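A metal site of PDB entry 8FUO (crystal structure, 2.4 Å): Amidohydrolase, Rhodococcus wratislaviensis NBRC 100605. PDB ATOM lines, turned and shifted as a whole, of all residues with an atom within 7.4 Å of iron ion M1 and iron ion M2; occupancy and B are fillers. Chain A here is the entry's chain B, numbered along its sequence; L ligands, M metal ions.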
ATOM      1  N   ASP A  25       2.099  22.705 -22.745  1.00  0.00           N
ATOM      2  CA  ASP A  25       2.335  21.328 -23.139  1.00  0.00           C
ATOM      3  C   ASP A  25       2.310  21.220 -24.667  1.00  0.00           C
ATOM      4  O   ASP A  25       1.242  21.196 -25.285  1.00  0.00           O
ATOM      5  CB  ASP A  25       1.290  20.383 -22.517  1.00  0.00           C
ATOM      6  CG  ASP A  25       1.591  18.947 -22.800  1.00  0.00           C
ATOM      7  OD1 ASP A  25       2.755  18.593 -22.723  1.00  0.00           O
ATOM      8  OD2 ASP A  25       0.673  18.173 -23.141  1.00  0.00           O
ATOM      9  N   ILE A  26       3.512  21.078 -25.248  1.00  0.00           N
ATOM     10  CA  ILE A  26       3.745  20.928 -26.687  1.00  0.00           C
ATOM     11  C   ILE A  26       4.715  19.782 -26.878  1.00  0.00           C
ATOM     12  O   ILE A  26       5.727  19.699 -26.176  1.00  0.00           O
ATOM     13  CB  ILE A  26       4.356  22.196 -27.310  1.00  0.00           C
ATOM     14  CG1 ILE A  26       3.417  23.384 -27.221  1.00  0.00           C
ATOM     15  CG2 ILE A  26       4.796  21.948 -28.762  1.00  0.00           C
ATOM     16  CD1 ILE A  26       4.161  24.676 -27.321  1.00  0.00           C
ATOM     17  N   HIS A  27       4.440  18.928 -27.872  1.00  0.00           N
ATOM     18  CA  HIS A  27       5.177  17.682 -28.068  1.00  0.00           C
ATOM     19  C   HIS A  27       6.009  17.705 -29.352  1.00  0.00           C
ATOM     20  O   HIS A  27       5.536  17.239 -30.417  1.00  0.00           O
ATOM     21  CB  HIS A  27       4.202  16.503 -28.054  1.00  0.00           C
ATOM     22  CG  HIS A  27       3.558  16.304 -26.726  1.00  0.00           C
ATOM     23  ND1 HIS A  27       4.283  16.291 -25.554  1.00  0.00           N
ATOM     24  CD2 HIS A  27       2.257  16.177 -26.354  1.00  0.00           C
ATOM     25  CE1 HIS A  27       3.466  16.129 -24.529  1.00  0.00           C
ATOM     26  NE2 HIS A  27       2.230  16.058 -24.993  1.00  0.00           N
ATOM     27  N   ALA A  71      -2.740   9.031 -32.831  1.00  0.00           N
ATOM     28  CA  ALA A  71      -3.410   9.939 -31.949  1.00  0.00           C
ATOM     29  C   ALA A  71      -2.947  11.307 -32.284  1.00  0.00           C
ATOM     30  O   ALA A  71      -2.915  12.159 -31.458  1.00  0.00           O
ATOM     31  CB  ALA A  71      -3.264   9.589 -30.492  1.00  0.00           C
ATOM     32  N   GLN A 106       7.553  19.404 -24.107  1.00  0.00           N
ATOM     33  CA  GLN A 106       7.545  18.164 -23.327  1.00  0.00           C
ATOM     34  C   GLN A 106       7.734  17.032 -24.333  1.00  0.00           C
ATOM     35  O   GLN A 106       6.779  16.442 -24.852  1.00  0.00           O
ATOM     36  CB  GLN A 106       6.264  18.010 -22.481  1.00  0.00           C
ATOM     37  CG  GLN A 106       5.885  19.277 -21.722  1.00  0.00           C
ATOM     38  CD  GLN A 106       4.899  19.034 -20.590  1.00  0.00           C
ATOM     39  OE1 GLN A 106       4.481  17.903 -20.356  1.00  0.00           O
ATOM     40  NE2 GLN A 106       4.505  20.097 -19.890  1.00  0.00           N
ATOM     41  N   LEU A 108       8.188  13.573 -25.541  1.00  0.00           N
ATOM     42  CA  LEU A 108       7.700  12.347 -24.924  1.00  0.00           C
ATOM     43  C   LEU A 108       8.380  11.081 -25.451  1.00  0.00           C
ATOM     44  O   LEU A 108       8.087   9.998 -24.941  1.00  0.00           O
ATOM     45  CB  LEU A 108       6.191  12.211 -25.160  1.00  0.00           C
ATOM     46  CG  LEU A 108       5.197  13.146 -24.464  1.00  0.00           C
ATOM     47  CD1 LEU A 108       3.788  12.614 -24.733  1.00  0.00           C
ATOM     48  CD2 LEU A 108       5.475  13.334 -22.943  1.00  0.00           C
ATOM     49  N   THR A 114       4.824   8.448 -30.556  1.00  0.00           N
ATOM     50  CA  THR A 114       3.929   9.371 -29.863  1.00  0.00           C
ATOM     51  C   THR A 114       4.257   9.492 -28.378  1.00  0.00           C
ATOM     52  O   THR A 114       4.417  10.608 -27.861  1.00  0.00           O
ATOM     53  CB  THR A 114       2.476   8.920 -30.052  1.00  0.00           C
ATOM     54  OG1 THR A 114       2.164   8.942 -31.442  1.00  0.00           O
ATOM     55  CG2 THR A 114       1.522   9.863 -29.313  1.00  0.00           C
ATOM     56  N   LEU A 115       4.356   8.371 -27.676  1.00  0.00           N
ATOM     57  CA  LEU A 115       4.593   8.366 -26.229  1.00  0.00           C
ATOM     58  C   LEU A 115       5.506   7.179 -25.918  1.00  0.00           C
ATOM     59  O   LEU A 115       5.052   6.032 -25.932  1.00  0.00           O
ATOM     60  CB  LEU A 115       3.269   8.282 -25.477  1.00  0.00           C
ATOM     61  CG  LEU A 115       3.245   8.111 -23.951  1.00  0.00           C
ATOM     62  CD1 LEU A 115       3.987   9.240 -23.242  1.00  0.00           C
ATOM     63  CD2 LEU A 115       1.793   8.014 -23.453  1.00  0.00           C
ATOM     64  N   HIS A 211       3.795  14.876 -16.687  1.00  0.00           N
ATOM     65  CA  HIS A 211       2.955  14.576 -17.841  1.00  0.00           C
ATOM     66  C   HIS A 211       2.436  13.135 -17.795  1.00  0.00           C
ATOM     67  O   HIS A 211       3.104  12.211 -17.307  1.00  0.00           O
ATOM     68  CB  HIS A 211       3.739  14.809 -19.137  1.00  0.00           C
ATOM     69  CG  HIS A 211       2.900  14.715 -20.358  1.00  0.00           C
ATOM     70  ND1 HIS A 211       2.693  13.527 -21.045  1.00  0.00           N
ATOM     71  CD2 HIS A 211       2.204  15.662 -21.036  1.00  0.00           C
ATOM     72  CE1 HIS A 211       1.905  13.750 -22.077  1.00  0.00           C
ATOM     73  NE2 HIS A 211       1.601  15.036 -22.099  1.00  0.00           N
ATOM     74  N   LEU A 212       1.219  12.983 -18.306  1.00  0.00           N
ATOM     75  CA  LEU A 212       0.584  11.688 -18.577  1.00  0.00           C
ATOM     76  C   LEU A 212       1.549  10.678 -19.194  1.00  0.00           C
ATOM     77  O   LEU A 212       2.169  10.946 -20.224  1.00  0.00           O
ATOM     78  CB  LEU A 212      -0.604  11.945 -19.516  1.00  0.00           C
ATOM     79  CG  LEU A 212      -1.443  10.926 -20.296  1.00  0.00           C
ATOM     80  CD1 LEU A 212      -2.721  11.616 -20.795  1.00  0.00           C
ATOM     81  CD2 LEU A 212      -0.709  10.285 -21.474  1.00  0.00           C
ATOM     82  N   HIS A 233      -7.605   5.653 -21.905  1.00  0.00           N
ATOM     83  CA  HIS A 233      -7.454   7.096 -21.944  1.00  0.00           C
ATOM     84  C   HIS A 233      -8.144   7.751 -20.737  1.00  0.00           C
ATOM     85  O   HIS A 233      -7.548   8.630 -20.090  1.00  0.00           O
ATOM     86  CB  HIS A 233      -7.975   7.632 -23.286  1.00  0.00           C
ATOM     87  CG  HIS A 233      -7.462   8.994 -23.623  1.00  0.00           C
ATOM     88  ND1 HIS A 233      -7.820   9.661 -24.787  1.00  0.00           N
ATOM     89  CD2 HIS A 233      -6.637   9.835 -22.959  1.00  0.00           C
ATOM     90  CE1 HIS A 233      -7.232  10.845 -24.821  1.00  0.00           C
ATOM     91  NE2 HIS A 233      -6.510  10.975 -23.721  1.00  0.00           N
ATOM     92  N   VAL A 264      -0.009  17.508 -15.624  1.00  0.00           N
ATOM     93  CA  VAL A 264      -0.173  17.911 -17.021  1.00  0.00           C
ATOM     94  C   VAL A 264      -0.924  16.804 -17.754  1.00  0.00           C
ATOM     95  O   VAL A 264      -0.458  15.660 -17.800  1.00  0.00           O
ATOM     96  CB  VAL A 264       1.165  18.202 -17.699  1.00  0.00           C
ATOM     97  CG1 VAL A 264       0.976  18.439 -19.210  1.00  0.00           C
ATOM     98  CG2 VAL A 264       1.864  19.358 -17.009  1.00  0.00           C
ATOM     99  N   GLU A 265      -2.065  17.162 -18.339  1.00  0.00           N
ATOM    100  CA  GLU A 265      -2.915  16.229 -19.062  1.00  0.00           C
ATOM    101  C   GLU A 265      -3.462  15.121 -18.149  1.00  0.00           C
ATOM    102  O   GLU A 265      -3.591  13.968 -18.543  1.00  0.00           O
ATOM    103  CB  GLU A 265      -2.159  15.633 -20.248  1.00  0.00           C
ATOM    104  CG  GLU A 265      -3.034  15.263 -21.382  1.00  0.00           C
ATOM    105  CD  GLU A 265      -2.229  15.153 -22.634  1.00  0.00           C
ATOM    106  OE1 GLU A 265      -1.269  15.940 -22.754  1.00  0.00           O
ATOM    107  OE2 GLU A 265      -2.520  14.261 -23.467  1.00  0.00           O
ATOM    108  N   SER A 307      -2.764  21.592 -15.776  1.00  0.00           N
ATOM    109  CA  SER A 307      -3.004  22.130 -17.106  1.00  0.00           C
ATOM    110  C   SER A 307      -4.402  21.705 -17.593  1.00  0.00           C
ATOM    111  O   SER A 307      -5.003  20.761 -17.080  1.00  0.00           O
ATOM    112  CB  SER A 307      -1.898  21.691 -18.056  1.00  0.00           C
ATOM    113  OG  SER A 307      -1.979  20.307 -18.392  1.00  0.00           O
ATOM    114  N   GLN A 309      -5.853  21.092 -20.977  1.00  0.00           N
ATOM    115  CA  GLN A 309      -6.076  20.074 -21.992  1.00  0.00           C
ATOM    116  C   GLN A 309      -6.002  18.677 -21.381  1.00  0.00           C
ATOM    117  O   GLN A 309      -5.146  18.414 -20.526  1.00  0.00           O
ATOM    118  CB  GLN A 309      -5.014  20.237 -23.090  1.00  0.00           C
ATOM    119  CG  GLN A 309      -5.320  19.532 -24.384  1.00  0.00           C
ATOM    120  CD  GLN A 309      -5.016  18.050 -24.344  1.00  0.00           C
ATOM    121  OE1 GLN A 309      -4.269  17.571 -23.491  1.00  0.00           O
ATOM    122  NE2 GLN A 309      -5.592  17.315 -25.293  1.00  0.00           N
ATOM    123  N   PRO A 310      -6.886  17.730 -21.789  1.00  0.00           N
ATOM    124  CA  PRO A 310      -8.046  17.931 -22.685  1.00  0.00           C
ATOM    125  C   PRO A 310      -9.253  18.452 -21.889  1.00  0.00           C
ATOM    126  O   PRO A 310      -9.757  17.715 -21.030  1.00  0.00           O
ATOM    127  CB  PRO A 310      -8.292  16.541 -23.254  1.00  0.00           C
ATOM    128  CG  PRO A 310      -7.813  15.596 -22.147  1.00  0.00           C
ATOM    129  CD  PRO A 310      -6.720  16.308 -21.421  1.00  0.00           C
ATOM    130  N   ALA A 335      -3.060  24.689 -21.905  1.00  0.00           N
ATOM    131  CA  ALA A 335      -2.200  23.919 -22.781  1.00  0.00           C
ATOM    132  C   ALA A 335      -2.959  23.595 -24.054  1.00  0.00           C
ATOM    133  O   ALA A 335      -4.186  23.515 -24.054  1.00  0.00           O
ATOM    134  CB  ALA A 335      -1.696  22.617 -22.116  1.00  0.00           C
ATOM    135  N   THR A 336      -2.224  23.382 -25.151  1.00  0.00           N
ATOM    136  CA  THR A 336      -2.852  22.895 -26.370  1.00  0.00           C
ATOM    137  C   THR A 336      -2.717  21.393 -26.555  1.00  0.00           C
ATOM    138  O   THR A 336      -3.614  20.772 -27.122  1.00  0.00           O
ATOM    139  CB  THR A 336      -2.287  23.581 -27.629  1.00  0.00           C
ATOM    140  OG1 THR A 336      -0.971  23.075 -27.971  1.00  0.00           O
ATOM    141  CG2 THR A 336      -2.277  25.088 -27.448  1.00  0.00           C
ATOM    142  N   ASP A 337      -1.610  20.810 -26.095  1.00  0.00           N
ATOM    143  CA  ASP A 337      -1.227  19.447 -26.418  1.00  0.00           C
ATOM    144  C   ASP A 337      -0.940  19.250 -27.914  1.00  0.00           C
ATOM    145  O   ASP A 337      -1.085  18.140 -28.425  1.00  0.00           O
ATOM    146  CB  ASP A 337      -2.295  18.438 -25.967  1.00  0.00           C
ATOM    147  CG  ASP A 337      -1.732  17.090 -25.685  1.00  0.00           C
ATOM    148  OD1 ASP A 337      -0.564  17.043 -25.259  1.00  0.00           O
ATOM    149  OD2 ASP A 337      -2.425  16.073 -25.895  1.00  0.00           O
ATOM    150  N   TYR A 338      -0.532  20.295 -28.621  1.00  0.00           N
ATOM    151  CA  TYR A 338      -0.169  20.133 -30.019  1.00  0.00           C
ATOM    152  C   TYR A 338       1.006  19.160 -30.140  1.00  0.00           C
ATOM    153  O   TYR A 338       1.982  19.268 -29.387  1.00  0.00           O
ATOM    154  CB  TYR A 338       0.237  21.468 -30.634  1.00  0.00           C
ATOM    155  CG  TYR A 338       0.661  21.367 -32.089  1.00  0.00           C
ATOM    156  CD1 TYR A 338      -0.245  21.617 -33.121  1.00  0.00           C
ATOM    157  CD2 TYR A 338       1.963  21.035 -32.422  1.00  0.00           C
ATOM    158  CE1 TYR A 338       0.136  21.517 -34.443  1.00  0.00           C
ATOM    159  CE2 TYR A 338       2.357  20.923 -33.746  1.00  0.00           C
ATOM    160  CZ  TYR A 338       1.448  21.171 -34.749  1.00  0.00           C
ATOM    161  OH  TYR A 338       1.857  21.067 -36.067  1.00  0.00           O
ATOM    162  N   PRO A 339       1.002  18.247 -31.134  1.00  0.00           N
ATOM    163  CA  PRO A 339       0.040  17.989 -32.221  1.00  0.00           C
ATOM    164  C   PRO A 339      -0.877  16.800 -32.006  1.00  0.00           C
ATOM    165  O   PRO A 339      -1.155  16.075 -32.968  1.00  0.00           O
ATOM    166  CB  PRO A 339       0.960  17.703 -33.410  1.00  0.00           C
ATOM    167  CG  PRO A 339       2.089  16.975 -32.782  1.00  0.00           C
ATOM    168  CD  PRO A 339       2.274  17.549 -31.378  1.00  0.00           C
ATOM    169  N   HIS A 340      -1.335  16.584 -30.769  1.00  0.00           N
ATOM    170  CA  HIS A 340      -2.159  15.417 -30.506  1.00  0.00           C
ATOM    171  C   HIS A 340      -3.593  15.664 -30.955  1.00  0.00           C
ATOM    172  O   HIS A 340      -4.024  16.814 -31.104  1.00  0.00           O
ATOM    173  CB  HIS A 340      -2.093  15.036 -29.030  1.00  0.00           C
ATOM    174  CG  HIS A 340      -0.799  14.408 -28.650  1.00  0.00           C
ATOM    175  ND1 HIS A 340      -0.578  13.822 -27.428  1.00  0.00           N
ATOM    176  CD2 HIS A 340       0.355  14.250 -29.355  1.00  0.00           C
ATOM    177  CE1 HIS A 340       0.659  13.331 -27.388  1.00  0.00           C
ATOM    178  NE2 HIS A 340       1.239  13.586 -28.548  1.00  0.00           N
ATOM    179  N   PHE A 341      -4.312  14.572 -31.186  1.00  0.00           N
ATOM    180  CA  PHE A 341      -5.589  14.660 -31.894  1.00  0.00           C
ATOM    181  C   PHE A 341      -6.629  15.433 -31.094  1.00  0.00           C
ATOM    182  O   PHE A 341      -7.490  16.101 -31.693  1.00  0.00           O
ATOM    183  CB  PHE A 341      -6.105  13.268 -32.231  1.00  0.00           C
ATOM    184  CG  PHE A 341      -6.912  12.637 -31.123  1.00  0.00           C
ATOM    185  CD1 PHE A 341      -6.288  11.931 -30.099  1.00  0.00           C
ATOM    186  CD2 PHE A 341      -8.289  12.789 -31.081  1.00  0.00           C
ATOM    187  CE1 PHE A 341      -7.026  11.360 -29.070  1.00  0.00           C
ATOM    188  CE2 PHE A 341      -9.038  12.238 -30.046  1.00  0.00           C
ATOM    189  CZ  PHE A 341      -8.407  11.525 -29.032  1.00  0.00           C
ATOM    190  N   ASP A 342      -6.589  15.357 -29.751  1.00  0.00           N
ATOM    191  CA  ASP A 342      -7.507  16.115 -28.905  1.00  0.00           C
ATOM    192  C   ASP A 342      -6.945  17.499 -28.540  1.00  0.00           C
ATOM    193  O   ASP A 342      -7.436  18.120 -27.585  1.00  0.00           O
ATOM    194  CB  ASP A 342      -7.897  15.315 -27.640  1.00  0.00           C
ATOM    195  CG  ASP A 342      -6.701  14.670 -26.896  1.00  0.00           C
ATOM    196  OD1 ASP A 342      -5.537  14.775 -27.378  1.00  0.00           O
ATOM    197  OD2 ASP A 342      -6.954  14.049 -25.826  1.00  0.00           O
ATOM    198  N   PHE A 343      -5.978  17.996 -29.319  1.00  0.00           N
ATOM    199  CA  PHE A 343      -5.506  19.376 -29.290  1.00  0.00           C
ATOM    200  C   PHE A 343      -6.575  20.368 -28.823  1.00  0.00           C
ATOM    201  O   PHE A 343      -7.734  20.267 -29.240  1.00  0.00           O
ATOM    202  CB  PHE A 343      -5.009  19.760 -30.689  1.00  0.00           C
ATOM    203  CG  PHE A 343      -4.785  21.235 -30.896  1.00  0.00           C
ATOM    204  CD1 PHE A 343      -5.795  22.044 -31.422  1.00  0.00           C
ATOM    205  CD2 PHE A 343      -3.533  21.806 -30.645  1.00  0.00           C
ATOM    206  CE1 PHE A 343      -5.574  23.406 -31.647  1.00  0.00           C
ATOM    207  CE2 PHE A 343      -3.307  23.164 -30.863  1.00  0.00           C
ATOM    208  CZ  PHE A 343      -4.343  23.964 -31.358  1.00  0.00           C
HETATM  209  C1  LIG L   1      -2.673  11.219 -25.871  1.00  0.00           C
HETATM  210  C2  LIG L   1      -1.877  10.817 -27.108  1.00  0.00           C
HETATM  211  C3  LIG L   1      -3.202   9.965 -25.181  1.00  0.00           C
HETATM  212  C4  LIG L   1      -3.860  12.135 -26.236  1.00  0.00           C
HETATM  213  N1  LIG L   1      -1.697  11.823 -24.970  1.00  0.00           N
HETATM  214  O1  LIG L   1      -0.971   9.828 -26.669  1.00  0.00           O
HETATM  215  O2  LIG L   1      -3.967   9.176 -26.076  1.00  0.00           O
HETATM  216  O3  LIG L   1      -3.519  13.497 -26.447  1.00  0.00           O
HETATM  217 FE    FE M   1      -1.530  14.132 -25.371  1.00  0.00          FE
HETATM  218 FE    FE M   2       0.486  16.089 -23.878  1.00  0.00          FE
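Within 4 Å of iron ion M2: Asp 25, His 27, His 211, Glu 265 and Asp 337. Along chain A the residues within 4 Å of iron ion M2 span positions 25 to 337.
Iron ion M2 is bound by OD1 of Asp 337 (2.0 Å), NE2 of His 27 (2.1 Å), OE1 of Glu 265 (2.1 Å), OD2 of Asp 25 (2.2 Å) and NE2 of His 211 (2.3 Å).
The backbone NH (N) of His 27 is in hydrogen-bond range of the backbone carbonyl oxygen (O) of Tyr 338 (2.9 Å). The side-chain carboxylate (OE1) of Glu 265 lies close to the side-chain amide oxygen (OE1) of Gln 309. The side-chain amide oxygen of Gln 106 lies close to the side-chain carboxylate of Asp 25 (3.0 Å). ND1 of His 27 is in hydrogen-bond range of O of Gln 106, at 2.6 Å. OD2 of Asp 337 lies close to OE1 of Gln 309, at 3.4 Å. The backbone NH (N) of Glu 265 is in hydrogen-bond range of the side-chain hydroxyl (OG) of Ser 307 (3.1 Å).
Iron ion M1 is bound by the side-chain carboxylate (OE2) of Glu 265 (2.1 Å), the side-chain carboxylate (OD2) of Asp 337 (2.2 Å), a ring nitrogen (ND1) of His 340 (2.3 Å), a nitrogen (N1) of the ligand (2.3 Å) and an oxygen (O3) of the ligand (2.3 Å). Iron ion M1 has five donor atoms within binding distance.
Of the 25 residues printed, 3 come within 4 Å of iron ion M1. Along chain A the residues within 4 Å of iron ion M1 span positions 265 to 340. The nearest printed residue that does not touch iron ion M1 is His 27 (4.2 Å).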
